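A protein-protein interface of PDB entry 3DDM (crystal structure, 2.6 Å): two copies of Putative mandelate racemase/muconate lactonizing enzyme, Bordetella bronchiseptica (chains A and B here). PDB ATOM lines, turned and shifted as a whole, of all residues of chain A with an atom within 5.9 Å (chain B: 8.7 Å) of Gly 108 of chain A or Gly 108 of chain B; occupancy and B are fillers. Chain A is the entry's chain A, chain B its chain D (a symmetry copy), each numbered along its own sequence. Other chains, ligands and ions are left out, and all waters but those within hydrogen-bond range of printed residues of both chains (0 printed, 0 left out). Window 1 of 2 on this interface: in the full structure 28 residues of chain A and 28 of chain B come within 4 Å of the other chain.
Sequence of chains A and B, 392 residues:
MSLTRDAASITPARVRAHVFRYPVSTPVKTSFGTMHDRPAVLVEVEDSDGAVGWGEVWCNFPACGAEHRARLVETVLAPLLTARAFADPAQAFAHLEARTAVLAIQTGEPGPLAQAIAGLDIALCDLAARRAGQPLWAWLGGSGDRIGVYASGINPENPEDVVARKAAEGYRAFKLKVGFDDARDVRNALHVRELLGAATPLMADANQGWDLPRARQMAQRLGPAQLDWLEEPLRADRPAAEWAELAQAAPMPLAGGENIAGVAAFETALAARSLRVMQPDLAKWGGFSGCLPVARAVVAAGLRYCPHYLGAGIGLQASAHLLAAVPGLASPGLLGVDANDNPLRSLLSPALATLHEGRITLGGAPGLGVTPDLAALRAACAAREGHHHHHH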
ATOM      1  N   ARG A  69      15.100  -2.481  18.424  1.00  0.00           N
ATOM      2  CA  ARG A  69      15.576  -3.174  17.244  1.00  0.00           C
ATOM      3  C   ARG A  69      15.412  -4.678  17.355  1.00  0.00           C
ATOM      4  O   ARG A  69      15.051  -5.340  16.384  1.00  0.00           O
ATOM      5  CB  ARG A  69      17.024  -2.782  16.984  1.00  0.00           C
ATOM      6  CG  ARG A  69      17.132  -1.344  16.502  1.00  0.00           C
ATOM      7  CD  ARG A  69      18.545  -0.792  16.590  1.00  0.00           C
ATOM      8  NE  ARG A  69      18.660   0.439  15.818  1.00  0.00           N
ATOM      9  CZ  ARG A  69      17.981   1.550  16.073  1.00  0.00           C
ATOM     10  NH1 ARG A  69      17.131   1.602  17.093  1.00  0.00           N
ATOM     11  NH2 ARG A  69      18.136   2.608  15.291  1.00  0.00           N
ATOM     12  N   LEU A 103       5.480   0.326   6.147  1.00  0.00           N
ATOM     13  CA  LEU A 103       5.570   0.464   7.592  1.00  0.00           C
ATOM     14  C   LEU A 103       6.662   1.491   7.933  1.00  0.00           C
ATOM     15  O   LEU A 103       6.580   2.194   8.946  1.00  0.00           O
ATOM     16  CB  LEU A 103       5.897  -0.891   8.218  1.00  0.00           C
ATOM     17  CG  LEU A 103       6.184  -0.876   9.715  1.00  0.00           C
ATOM     18  CD1 LEU A 103       4.905  -0.501  10.470  1.00  0.00           C
ATOM     19  CD2 LEU A 103       6.723  -2.230  10.149  1.00  0.00           C
ATOM     20  N   ALA A 104       7.686   1.583   7.087  1.00  0.00           N
ATOM     21  CA  ALA A 104       8.767   2.537   7.313  1.00  0.00           C
ATOM     22  C   ALA A 104       8.192   3.944   7.202  1.00  0.00           C
ATOM     23  O   ALA A 104       8.461   4.814   8.035  1.00  0.00           O
ATOM     24  CB  ALA A 104       9.860   2.339   6.288  1.00  0.00           C
ATOM     25  N   ILE A 105       7.387   4.158   6.169  1.00  0.00           N
ATOM     26  CA  ILE A 105       6.765   5.448   5.958  1.00  0.00           C
ATOM     27  C   ILE A 105       5.879   5.823   7.148  1.00  0.00           C
ATOM     28  O   ILE A 105       6.059   6.876   7.760  1.00  0.00           O
ATOM     29  CB  ILE A 105       5.923   5.438   4.660  1.00  0.00           C
ATOM     30  CG1 ILE A 105       6.854   5.382   3.443  1.00  0.00           C
ATOM     31  CG2 ILE A 105       5.015   6.671   4.605  1.00  0.00           C
ATOM     32  CD1 ILE A 105       6.132   5.168   2.116  1.00  0.00           C
ATOM     33  N   GLN A 106       4.935   4.949   7.474  1.00  0.00           N
ATOM     34  CA  GLN A 106       3.999   5.171   8.571  1.00  0.00           C
ATOM     35  C   GLN A 106       4.636   5.519   9.898  1.00  0.00           C
ATOM     36  O   GLN A 106       4.056   6.240  10.695  1.00  0.00           O
ATOM     37  CB  GLN A 106       3.125   3.930   8.774  1.00  0.00           C
ATOM     38  CG  GLN A 106       1.738   4.023   8.149  1.00  0.00           C
ATOM     39  CD  GLN A 106       0.753   4.811   9.007  1.00  0.00           C
ATOM     40  OE1 GLN A 106       0.322   4.346  10.071  1.00  0.00           O
ATOM     41  NE2 GLN A 106       0.398   6.010   8.551  1.00  0.00           N
ATOM     42  N   THR A 107       5.834   5.013  10.133  1.00  0.00           N
ATOM     43  CA  THR A 107       6.483   5.235  11.406  1.00  0.00           C
ATOM     44  C   THR A 107       7.712   6.118  11.365  1.00  0.00           C
ATOM     45  O   THR A 107       8.148   6.620  12.405  1.00  0.00           O
ATOM     46  CB  THR A 107       6.884   3.893  12.014  1.00  0.00           C
ATOM     47  OG1 THR A 107       7.880   3.280  11.191  1.00  0.00           O
ATOM     48  CG2 THR A 107       5.687   2.961  12.071  1.00  0.00           C
ATOM     49  N   GLY A 108       8.275   6.308  10.178  1.00  0.00           N
ATOM     50  CA  GLY A 108       9.468   7.119  10.078  1.00  0.00           C
ATOM     51  C   GLY A 108      10.649   6.390  10.693  1.00  0.00           C
ATOM     52  O   GLY A 108      11.533   7.007  11.302  1.00  0.00           O
ATOM     53  N   GLU A 109      10.655   5.064  10.545  1.00  0.00           N
ATOM     54  CA  GLU A 109      11.732   4.223  11.059  1.00  0.00           C
ATOM     55  C   GLU A 109      12.489   3.516   9.929  1.00  0.00           C
ATOM     56  O   GLU A 109      12.662   2.305   9.947  1.00  0.00           O
ATOM     57  CB  GLU A 109      11.179   3.192  12.048  1.00  0.00           C
ATOM     58  CG  GLU A 109      10.667   3.813  13.342  1.00  0.00           C
ATOM     59  CD  GLU A 109      10.284   2.785  14.408  1.00  0.00           C
ATOM     60  OE1 GLU A 109      10.888   1.692  14.420  1.00  0.00           O
ATOM     61  OE2 GLU A 109       9.398   3.080  15.246  1.00  0.00           O
ATOM     62  N   PRO A 110      12.956   4.274   8.924  1.00  0.00           N
ATOM     63  CA  PRO A 110      13.682   3.606   7.843  1.00  0.00           C
ATOM     64  C   PRO A 110      14.986   3.018   8.373  1.00  0.00           C
ATOM     65  O   PRO A 110      15.502   2.034   7.831  1.00  0.00           O
ATOM     66  CB  PRO A 110      13.922   4.732   6.848  1.00  0.00           C
ATOM     67  CG  PRO A 110      14.095   5.927   7.742  1.00  0.00           C
ATOM     68  CD  PRO A 110      12.980   5.740   8.747  1.00  0.00           C
ATOM     69  N   GLY A 111      15.500   3.633   9.438  1.00  0.00           N
ATOM     70  CA  GLY A 111      16.741   3.195  10.060  1.00  0.00           C
ATOM     71  C   GLY A 111      16.619   1.910  10.863  1.00  0.00           C
ATOM     72  O   GLY A 111      17.253   0.912  10.528  1.00  0.00           O
ATOM     73  N   PRO A 112      15.824   1.903  11.944  1.00  0.00           N
ATOM     74  CA  PRO A 112      15.664   0.694  12.756  1.00  0.00           C
ATOM     75  C   PRO A 112      15.354  -0.528  11.892  1.00  0.00           C
ATOM     76  O   PRO A 112      15.956  -1.594  12.060  1.00  0.00           O
ATOM     77  CB  PRO A 112      14.505   1.057  13.675  1.00  0.00           C
ATOM     78  CG  PRO A 112      14.728   2.511  13.897  1.00  0.00           C
ATOM     79  CD  PRO A 112      15.047   3.020  12.511  1.00  0.00           C
ATOM     80  N   GLN A 115      18.340  -1.602   9.668  1.00  0.00           N
ATOM     81  CA  GLN A 115      19.319  -2.197  10.555  1.00  0.00           C
ATOM     82  C   GLN A 115      18.926  -3.623  10.942  1.00  0.00           C
ATOM     83  O   GLN A 115      19.740  -4.561  10.859  1.00  0.00           O
ATOM     84  CB  GLN A 115      19.479  -1.305  11.789  1.00  0.00           C
ATOM     85  CG  GLN A 115      20.345  -0.068  11.532  1.00  0.00           C
ATOM     86  CD  GLN A 115      19.772   1.222  12.119  1.00  0.00           C
ATOM     87  OE1 GLN A 115      19.338   1.267  13.270  1.00  0.00           O
ATOM     88  NE2 GLN A 115      19.789   2.280  11.326  1.00  0.00           N
ATOM     89  N   TRP B  58       2.580   9.958  19.563  1.00  0.00           N
ATOM     90  CA  TRP B  58       2.040   8.997  18.603  1.00  0.00           C
ATOM     91  C   TRP B  58       2.857   7.713  18.652  1.00  0.00           C
ATOM     92  O   TRP B  58       4.082   7.757  18.680  1.00  0.00           O
ATOM     93  CB  TRP B  58       2.101   9.565  17.190  1.00  0.00           C
ATOM     94  CG  TRP B  58       1.539   8.649  16.134  1.00  0.00           C
ATOM     95  CD1 TRP B  58       0.257   8.617  15.686  1.00  0.00           C
ATOM     96  CD2 TRP B  58       2.254   7.657  15.375  1.00  0.00           C
ATOM     97  NE1 TRP B  58       0.125   7.685  14.695  1.00  0.00           N
ATOM     98  CE2 TRP B  58       1.334   7.077  14.481  1.00  0.00           C
ATOM     99  CE3 TRP B  58       3.585   7.204  15.363  1.00  0.00           C
ATOM    100  CZ2 TRP B  58       1.695   6.065  13.579  1.00  0.00           C
ATOM    101  CZ3 TRP B  58       3.943   6.195  14.463  1.00  0.00           C
ATOM    102  CH2 TRP B  58       3.002   5.641  13.587  1.00  0.00           C
ATOM    103  N   PHE B  61       2.218   2.470  15.570  1.00  0.00           N
ATOM    104  CA  PHE B  61       3.073   1.541  14.847  1.00  0.00           C
ATOM    105  C   PHE B  61       4.552   1.890  15.040  1.00  0.00           C
ATOM    106  O   PHE B  61       4.912   3.060  15.190  1.00  0.00           O
ATOM    107  CB  PHE B  61       2.746   1.552  13.347  1.00  0.00           C
ATOM    108  CG  PHE B  61       1.295   1.300  13.028  1.00  0.00           C
ATOM    109  CD1 PHE B  61       0.362   2.341  13.076  1.00  0.00           C
ATOM    110  CD2 PHE B  61       0.853   0.018  12.684  1.00  0.00           C
ATOM    111  CE1 PHE B  61      -0.991   2.111  12.787  1.00  0.00           C
ATOM    112  CE2 PHE B  61      -0.499  -0.224  12.392  1.00  0.00           C
ATOM    113  CZ  PHE B  61      -1.421   0.828  12.446  1.00  0.00           C
ATOM    114  N   PRO B  62       5.420   0.865  15.083  1.00  0.00           N
ATOM    115  CA  PRO B  62       4.971  -0.525  14.960  1.00  0.00           C
ATOM    116  C   PRO B  62       4.291  -0.895  16.277  1.00  0.00           C
ATOM    117  O   PRO B  62       4.113  -0.035  17.142  1.00  0.00           O
ATOM    118  CB  PRO B  62       6.272  -1.284  14.712  1.00  0.00           C
ATOM    119  CG  PRO B  62       7.268  -0.495  15.493  1.00  0.00           C
ATOM    120  CD  PRO B  62       6.890   0.939  15.186  1.00  0.00           C
ATOM    121  N   HIS B  68      10.127   2.257  23.088  1.00  0.00           N
ATOM    122  CA  HIS B  68      11.253   2.984  22.517  1.00  0.00           C
ATOM    123  C   HIS B  68      11.010   4.491  22.542  1.00  0.00           C
ATOM    124  O   HIS B  68      11.880   5.257  22.953  1.00  0.00           O
ATOM    125  CB  HIS B  68      11.516   2.512  21.081  1.00  0.00           C
ATOM    126  CG  HIS B  68      12.658   3.216  20.419  1.00  0.00           C
ATOM    127  ND1 HIS B  68      13.904   3.319  20.997  1.00  0.00           N
ATOM    128  CD2 HIS B  68      12.733   3.888  19.246  1.00  0.00           C
ATOM    129  CE1 HIS B  68      14.696   4.028  20.213  1.00  0.00           C
ATOM    130  NE2 HIS B  68      14.009   4.386  19.144  1.00  0.00           N
ATOM    131  N   ARG B  69       9.829   4.918  22.106  1.00  0.00           N
ATOM    132  CA  ARG B  69       9.495   6.336  22.096  1.00  0.00           C
ATOM    133  C   ARG B  69       9.555   6.929  23.504  1.00  0.00           C
ATOM    134  O   ARG B  69      10.060   8.040  23.700  1.00  0.00           O
ATOM    135  CB  ARG B  69       8.117   6.534  21.450  1.00  0.00           C
ATOM    136  CG  ARG B  69       8.192   6.422  19.923  1.00  0.00           C
ATOM    137  CD  ARG B  69       6.909   5.931  19.271  1.00  0.00           C
ATOM    138  NE  ARG B  69       7.008   5.971  17.813  1.00  0.00           N
ATOM    139  CZ  ARG B  69       7.712   5.114  17.072  1.00  0.00           C
ATOM    140  NH1 ARG B  69       8.384   4.116  17.639  1.00  0.00           N
ATOM    141  NH2 ARG B  69       7.777   5.280  15.755  1.00  0.00           N
ATOM    142  N   THR B 100      18.872  17.326  17.765  1.00  0.00           N
ATOM    143  CA  THR B 100      18.749  15.908  17.455  1.00  0.00           C
ATOM    144  C   THR B 100      18.783  15.692  15.950  1.00  0.00           C
ATOM    145  O   THR B 100      18.611  14.572  15.469  1.00  0.00           O
ATOM    146  CB  THR B 100      17.441  15.292  18.046  1.00  0.00           C
ATOM    147  OG1 THR B 100      16.292  15.892  17.438  1.00  0.00           O
ATOM    148  CG2 THR B 100      17.383  15.511  19.543  1.00  0.00           C
ATOM    149  N   ALA B 101      19.019  16.773  15.212  1.00  0.00           N
ATOM    150  CA  ALA B 101      19.087  16.699  13.758  1.00  0.00           C
ATOM    151  C   ALA B 101      20.072  15.612  13.326  1.00  0.00           C
ATOM    152  O   ALA B 101      19.687  14.651  12.653  1.00  0.00           O
ATOM    153  CB  ALA B 101      19.495  18.043  13.181  1.00  0.00           C
ATOM    154  N   VAL B 102      21.335  15.755  13.719  1.00  0.00           N
ATOM    155  CA  VAL B 102      22.349  14.766  13.371  1.00  0.00           C
ATOM    156  C   VAL B 102      21.982  13.375  13.909  1.00  0.00           C
ATOM    157  O   VAL B 102      22.051  12.381  13.177  1.00  0.00           O
ATOM    158  CB  VAL B 102      23.758  15.177  13.903  1.00  0.00           C
ATOM    159  CG1 VAL B 102      24.757  14.055  13.652  1.00  0.00           C
ATOM    160  CG2 VAL B 102      24.233  16.443  13.204  1.00  0.00           C
ATOM    161  N   LEU B 103      21.590  13.289  15.175  1.00  0.00           N
ATOM    162  CA  LEU B 103      21.216  11.991  15.730  1.00  0.00           C
ATOM    163  C   LEU B 103      20.192  11.313  14.818  1.00  0.00           C
ATOM    164  O   LEU B 103      20.247  10.102  14.587  1.00  0.00           O
ATOM    165  CB  LEU B 103      20.622  12.162  17.124  1.00  0.00           C
ATOM    166  CG  LEU B 103      20.152  10.885  17.817  1.00  0.00           C
ATOM    167  CD1 LEU B 103      21.324   9.924  17.973  1.00  0.00           C
ATOM    168  CD2 LEU B 103      19.534  11.238  19.170  1.00  0.00           C
ATOM    169  N   ALA B 104      19.265  12.108  14.295  1.00  0.00           N
ATOM    170  CA  ALA B 104      18.222  11.602  13.408  1.00  0.00           C
ATOM    171  C   ALA B 104      18.818  10.975  12.153  1.00  0.00           C
ATOM    172  O   ALA B 104      18.280   9.999  11.625  1.00  0.00           O
ATOM    173  CB  ALA B 104      17.258  12.736  13.027  1.00  0.00           C
ATOM    174  N   ILE B 105      19.927  11.545  11.679  1.00  0.00           N
ATOM    175  CA  ILE B 105      20.614  11.051  10.485  1.00  0.00           C
ATOM    176  C   ILE B 105      21.445   9.795  10.789  1.00  0.00           C
ATOM    177  O   ILE B 105      21.521   8.886   9.970  1.00  0.00           O
ATOM    178  CB  ILE B 105      21.561  12.116   9.906  1.00  0.00           C
ATOM    179  CG1 ILE B 105      20.761  13.320   9.405  1.00  0.00           C
ATOM    180  CG2 ILE B 105      22.387  11.516   8.777  1.00  0.00           C
ATOM    181  CD1 ILE B 105      21.614  14.451   8.849  1.00  0.00           C
ATOM    182  N   GLN B 106      22.063   9.756  11.964  1.00  0.00           N
ATOM    183  CA  GLN B 106      22.885   8.624  12.374  1.00  0.00           C
ATOM    184  C   GLN B 106      22.071   7.360  12.581  1.00  0.00           C
ATOM    185  O   GLN B 106      22.472   6.266  12.190  1.00  0.00           O
ATOM    186  CB  GLN B 106      23.586   8.930  13.703  1.00  0.00           C
ATOM    187  CG  GLN B 106      24.884   9.690  13.627  1.00  0.00           C
ATOM    188  CD  GLN B 106      26.018   8.838  13.099  1.00  0.00           C
ATOM    189  OE1 GLN B 106      26.162   7.674  13.478  1.00  0.00           O
ATOM    190  NE2 GLN B 106      26.848   9.421  12.231  1.00  0.00           N
ATOM    191  N   THR B 107      20.927   7.531  13.225  1.00  0.00           N
ATOM    192  CA  THR B 107      20.053   6.419  13.582  1.00  0.00           C
ATOM    193  C   THR B 107      18.940   6.138  12.600  1.00  0.00           C
ATOM    194  O   THR B 107      18.339   5.071  12.650  1.00  0.00           O
ATOM    195  CB  THR B 107      19.390   6.685  14.927  1.00  0.00           C
ATOM    196  OG1 THR B 107      18.458   7.763  14.771  1.00  0.00           O
ATOM    197  CG2 THR B 107      20.419   7.082  15.956  1.00  0.00           C
ATOM    198  N   GLY B 108      18.648   7.100  11.728  1.00  0.00           N
ATOM    199  CA  GLY B 108      17.583   6.919  10.756  1.00  0.00           C
ATOM    200  C   GLY B 108      16.224   6.904  11.428  1.00  0.00           C
ATOM    201  O   GLY B 108      15.284   6.280  10.950  1.00  0.00           O
ATOM    202  N   GLU B 109      16.113   7.613  12.545  1.00  0.00           N
ATOM    203  CA  GLU B 109      14.862   7.643  13.282  1.00  0.00           C
ATOM    204  C   GLU B 109      14.132   8.975  13.246  1.00  0.00           C
ATOM    205  O   GLU B 109      13.696   9.479  14.279  1.00  0.00           O
ATOM    206  CB  GLU B 109      15.103   7.212  14.735  1.00  0.00           C
ATOM    207  CG  GLU B 109      15.498   5.750  14.867  1.00  0.00           C
ATOM    208  CD  GLU B 109      15.597   5.285  16.309  1.00  0.00           C
ATOM    209  OE1 GLU B 109      14.708   5.638  17.107  1.00  0.00           O
ATOM    210  OE2 GLU B 109      16.552   4.554  16.643  1.00  0.00           O
ATOM    211  N   PRO B 110      13.984   9.568  12.051  1.00  0.00           N
ATOM    212  CA  PRO B 110      13.269  10.847  12.015  1.00  0.00           C
ATOM    213  C   PRO B 110      11.901  10.754  12.713  1.00  0.00           C
ATOM    214  O   PRO B 110      11.533  11.637  13.492  1.00  0.00           O
ATOM    215  CB  PRO B 110      13.154  11.134  10.515  1.00  0.00           C
ATOM    216  CG  PRO B 110      13.254   9.756   9.871  1.00  0.00           C
ATOM    217  CD  PRO B 110      14.340   9.130  10.687  1.00  0.00           C
ATOM    218  N   GLY B 111      11.166   9.674  12.457  1.00  0.00           N
ATOM    219  CA  GLY B 111       9.857   9.507  13.068  1.00  0.00           C
ATOM    220  C   GLY B 111       9.848   9.481  14.590  1.00  0.00           C
ATOM    221  O   GLY B 111       9.266  10.359  15.220  1.00  0.00           O
ATOM    222  N   PRO B 112      10.468   8.468  15.213  1.00  0.00           N
ATOM    223  CA  PRO B 112      10.520   8.353  16.669  1.00  0.00           C
ATOM    224  C   PRO B 112      10.934   9.666  17.350  1.00  0.00           C
ATOM    225  O   PRO B 112      10.381  10.041  18.381  1.00  0.00           O
ATOM    226  CB  PRO B 112      11.547   7.239  16.885  1.00  0.00           C
ATOM    227  CG  PRO B 112      11.308   6.350  15.722  1.00  0.00           C
ATOM    228  CD  PRO B 112      11.160   7.334  14.575  1.00  0.00           C
ATOM    229  N   LEU B 113      11.916  10.359  16.787  1.00  0.00           N
ATOM    230  CA  LEU B 113      12.357  11.605  17.377  1.00  0.00           C
ATOM    231  C   LEU B 113      11.280  12.664  17.213  1.00  0.00           C
ATOM    232  O   LEU B 113      10.946  13.362  18.166  1.00  0.00           O
ATOM    233  CB  LEU B 113      13.679  12.051  16.751  1.00  0.00           C
ATOM    234  CG  LEU B 113      14.887  11.241  17.261  1.00  0.00           C
ATOM    235  CD1 LEU B 113      16.138  11.526  16.416  1.00  0.00           C
ATOM    236  CD2 LEU B 113      15.138  11.584  18.720  1.00  0.00           C
ATOM    237  N   ALA B 114      10.721  12.772  16.011  1.00  0.00           N
ATOM    238  CA  ALA B 114       9.668  13.756  15.750  1.00  0.00           C
ATOM    239  C   ALA B 114       8.467  13.513  16.686  1.00  0.00           C
ATOM    240  O   ALA B 114       7.947  14.442  17.320  1.00  0.00           O
ATOM    241  CB  ALA B 114       9.224  13.673  14.299  1.00  0.00           C
ATOM    242  N   GLN B 115       8.047  12.257  16.770  1.00  0.00           N
ATOM    243  CA  GLN B 115       6.933  11.863  17.609  1.00  0.00           C
ATOM    244  C   GLN B 115       7.190  12.147  19.097  1.00  0.00           C
ATOM    245  O   GLN B 115       6.286  12.568  19.830  1.00  0.00           O
ATOM    246  CB  GLN B 115       6.643  10.379  17.374  1.00  0.00           C
ATOM    247  CG  GLN B 115       5.979  10.109  16.043  1.00  0.00           C
ATOM    248  CD  GLN B 115       6.510   8.881  15.331  1.00  0.00           C
ATOM    249  OE1 GLN B 115       6.833   7.869  15.953  1.00  0.00           O
ATOM    250  NE2 GLN B 115       6.579   8.959  14.007  1.00  0.00           N
ATOM    251  N   GLU B 258      -0.949  12.657   7.513  1.00  0.00           N
ATOM    252  CA  GLU B 258      -0.607  11.709   8.575  1.00  0.00           C
ATOM    253  C   GLU B 258       0.852  11.265   8.443  1.00  0.00           C
ATOM    254  O   GLU B 258       1.529  11.023   9.437  1.00  0.00           O
ATOM    255  CB  GLU B 258      -1.569  10.501   8.487  1.00  0.00           C
ATOM    256  CG  GLU B 258      -1.184   9.220   9.246  1.00  0.00           C
ATOM    257  CD  GLU B 258      -1.119   9.375  10.775  1.00  0.00           C
ATOM    258  OE1 GLU B 258      -0.759   8.379  11.462  1.00  0.00           O
ATOM    259  OE2 GLU B 258      -1.422  10.482  11.293  1.00  0.00           O
ATOM    260  N   ASN B 259       1.335  11.190   7.207  1.00  0.00           N
ATOM    261  CA  ASN B 259       2.702  10.760   6.926  1.00  0.00           C
ATOM    262  C   ASN B 259       3.597  11.822   6.308  1.00  0.00           C
ATOM    263  O   ASN B 259       4.526  11.510   5.577  1.00  0.00           O
ATOM    264  CB  ASN B 259       2.680   9.526   6.028  1.00  0.00           C
ATOM    265  CG  ASN B 259       2.102   8.319   6.729  1.00  0.00           C
ATOM    266  OD1 ASN B 259       1.239   7.631   6.189  1.00  0.00           O
ATOM    267  ND2 ASN B 259       2.576   8.055   7.943  1.00  0.00           N
ATOM    268  N   ALA B 261       5.969  15.214   7.348  1.00  0.00           N
ATOM    269  CA  ALA B 261       6.596  15.833   8.516  1.00  0.00           C
ATOM    270  C   ALA B 261       7.608  16.893   8.131  1.00  0.00           C
ATOM    271  O   ALA B 261       8.372  16.724   7.177  1.00  0.00           O
ATOM    272  CB  ALA B 261       7.271  14.778   9.375  1.00  0.00           C
ATOM    273  N   LYS B 284       2.286  13.438  16.160  1.00  0.00           N
ATOM    274  CA  LYS B 284       3.265  12.728  15.336  1.00  0.00           C
ATOM    275  C   LYS B 284       4.388  13.668  14.874  1.00  0.00           C
ATOM    276  O   LYS B 284       5.527  13.245  14.698  1.00  0.00           O
ATOM    277  CB  LYS B 284       2.562  12.093  14.136  1.00  0.00           C
ATOM    278  CG  LYS B 284       3.166  10.784  13.682  1.00  0.00           C
ATOM    279  CD  LYS B 284       2.219  10.060  12.725  1.00  0.00           C
ATOM    280  CE  LYS B 284       2.960   9.013  11.902  1.00  0.00           C
ATOM    281  NZ  LYS B 284       2.111   8.424  10.834  1.00  0.00           N
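Of the 25 printed residues of chain B, 14 touch a printed residue of chain A. Hydrophobic or aromatic side chains of chain B that line the printed part of chain A: Trp 58, Phe 61, Pro 62, Pro 110 and Pro 112. Of the 12 printed residues of chain A, 10 touch a printed residue of chain B. Among the printed residues, 29 pairs touch across the chains. Among the printed residues, Asp or Glu carboxylates within 4 Å of a Lys or Arg side-chain nitrogen of the other chain: Arg 69 of chain A with Glu 109 of chain B (2.9 Å) and Glu 109 of chain A with Arg 69 of chain B (2.8 Å).
NZ of Lys 284 of chain B lies within salt-bridge range of OE1 of Glu 258 of chain B, at 2.9 Å. The side-chain hydroxyl of Thr 107 of chain A sits close to the backbone NH of Glu 109 of chain A (3.4 Å). The side-chain amide nitrogen of Asn 259 of chain B lies close to the side-chain amino group of Lys 284 of chain B (3.0 Å). O of Ala 104 of chain A lies within hydrogen-bond range of N of Glu 109 of chain A (3.3 Å).
NE2 of Gln 115 of chain A lies within hydrogen-bond range of O of Thr 107 of chain B, at 3.4 Å. OE2 of Glu 109 of chain A lies within salt-bridge range of NH2 of Arg 69 of chain B. The backbone carbonyl oxygen (O) of Gly 108 of chain A is in hydrogen-bond range of the backbone NH (N) of Gly 111 of chain B (2.9 Å). The side-chain amide oxygen of Asn 259 of chain B lies within hydrogen-bond range of the side-chain amide nitrogen of Gln 106 of chain A, 3.0 Å away. O of Thr 107 of chain A sits at hydrogen-bond distance from NE2 of Gln 115 of chain B (3.2 Å). The backbone NH of Gly 111 of chain A lies within hydrogen-bond range of the backbone carbonyl oxygen of Gly 108 of chain B. The guanidinium group (NH2) of Arg 69 of chain A is in salt-bridge range of the side-chain carboxylate (OE2) of Glu 109 of chain B (2.9 Å). The side-chain amino group of Lys 284 of chain B sits at hydrogen-bond distance from the backbone carbonyl oxygen of Gln 106 of chain A.
Gly 108 of chain A touches Pro 110 of chain B, and with the chains exchanged Pro 110 of chain A touches Gly 108 of chain B. Gly 108 of chain A touches Gly 111 of chain B, and with the chains exchanged Gly 111 of chain A touches Gly 108 of chain B. Glu 109 of chain A touches Pro 112 of chain B, and with the chains exchanged Pro 112 of chain A touches Glu 109 of chain B. Of the 29 pairs that touch across the chains among the printed residues, 19 have their exchanged pair printed and touching as well.
Of the printed residues of chain B, Arg 69 of chain A touches Thr 107 and Glu 109. Of the printed residues of chain B, Thr 107 of chain A touches Phe 61 (3.2 Å), Pro 62 (3.7 Å), Arg 69 (3.6 Å), Gly 111 (3.4 Å), Pro 112 (3.8 Å) and Gln 115 (3.2 Å). Gly 108 of chain A touches just these residues of chain B: Gly 108, Glu 109, Pro 110, Gly 111 and Pro 112. Printed residues of chain A within 4 Å of Gly 108 of chain B: Gly 108, Pro 110, Gly 111 and Pro 112. Printed residues of chain A within 4 Å of Glu 258 of chain B: Gln 106 (3.6 Å). The nearest printed residue of chain A that does not touch Glu 109 of chain B is Gly 111 of chain A (5.1 Å).
Among the printed residues, pairs that only touch across the chains: Arg 69 of chain A with Thr 107 of chain B (3.6 Å), Ile 105 of chain A with Asn 259 of chain B (3.7 Å), Gln 106 of chain A with Trp 58 of chain B (3.1 Å), Gln 106 of chain A with Phe 61 of chain B (3.6 Å), Gln 106 of chain A with Glu 258 of chain B (3.6 Å), Thr 107 of chain A with Phe 61 of chain B (3.2 Å), Thr 107 of chain A with Pro 62 of chain B (3.7 Å), Thr 107 of chain A with Arg 69 of chain B (3.6 Å), Thr 107 of chain A with Gly 111 of chain B (3.4 Å), Thr 107 of chain A with Pro 112 of chain B (3.8 Å), Gly 108 of chain A with Gly 108 of chain B (3.8 Å), Gly 108 of chain A with Glu 109 of chain B (3.8 Å), Gly 108 of chain A with Pro 110 of chain B (3.5 Å), Gly 108 of chain A with Pro 112 of chain B (3.3 Å), Glu 109 of chain A with Pro 62 of chain B (3.3 Å), Glu 109 of chain A with Pro 112 of chain B (3.5 Å), Pro 110 of chain A with Gly 108 of chain B (3.2 Å), Gly 111 of chain A with Thr 107 of chain B (3.6 Å), Pro 112 of chain A with Thr 107 of chain B (3.9 Å), Pro 112 of chain A with Gly 108 of chain B (3.6 Å) and Pro 112 of chain A with Glu 109 of chain B (3.5 Å).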
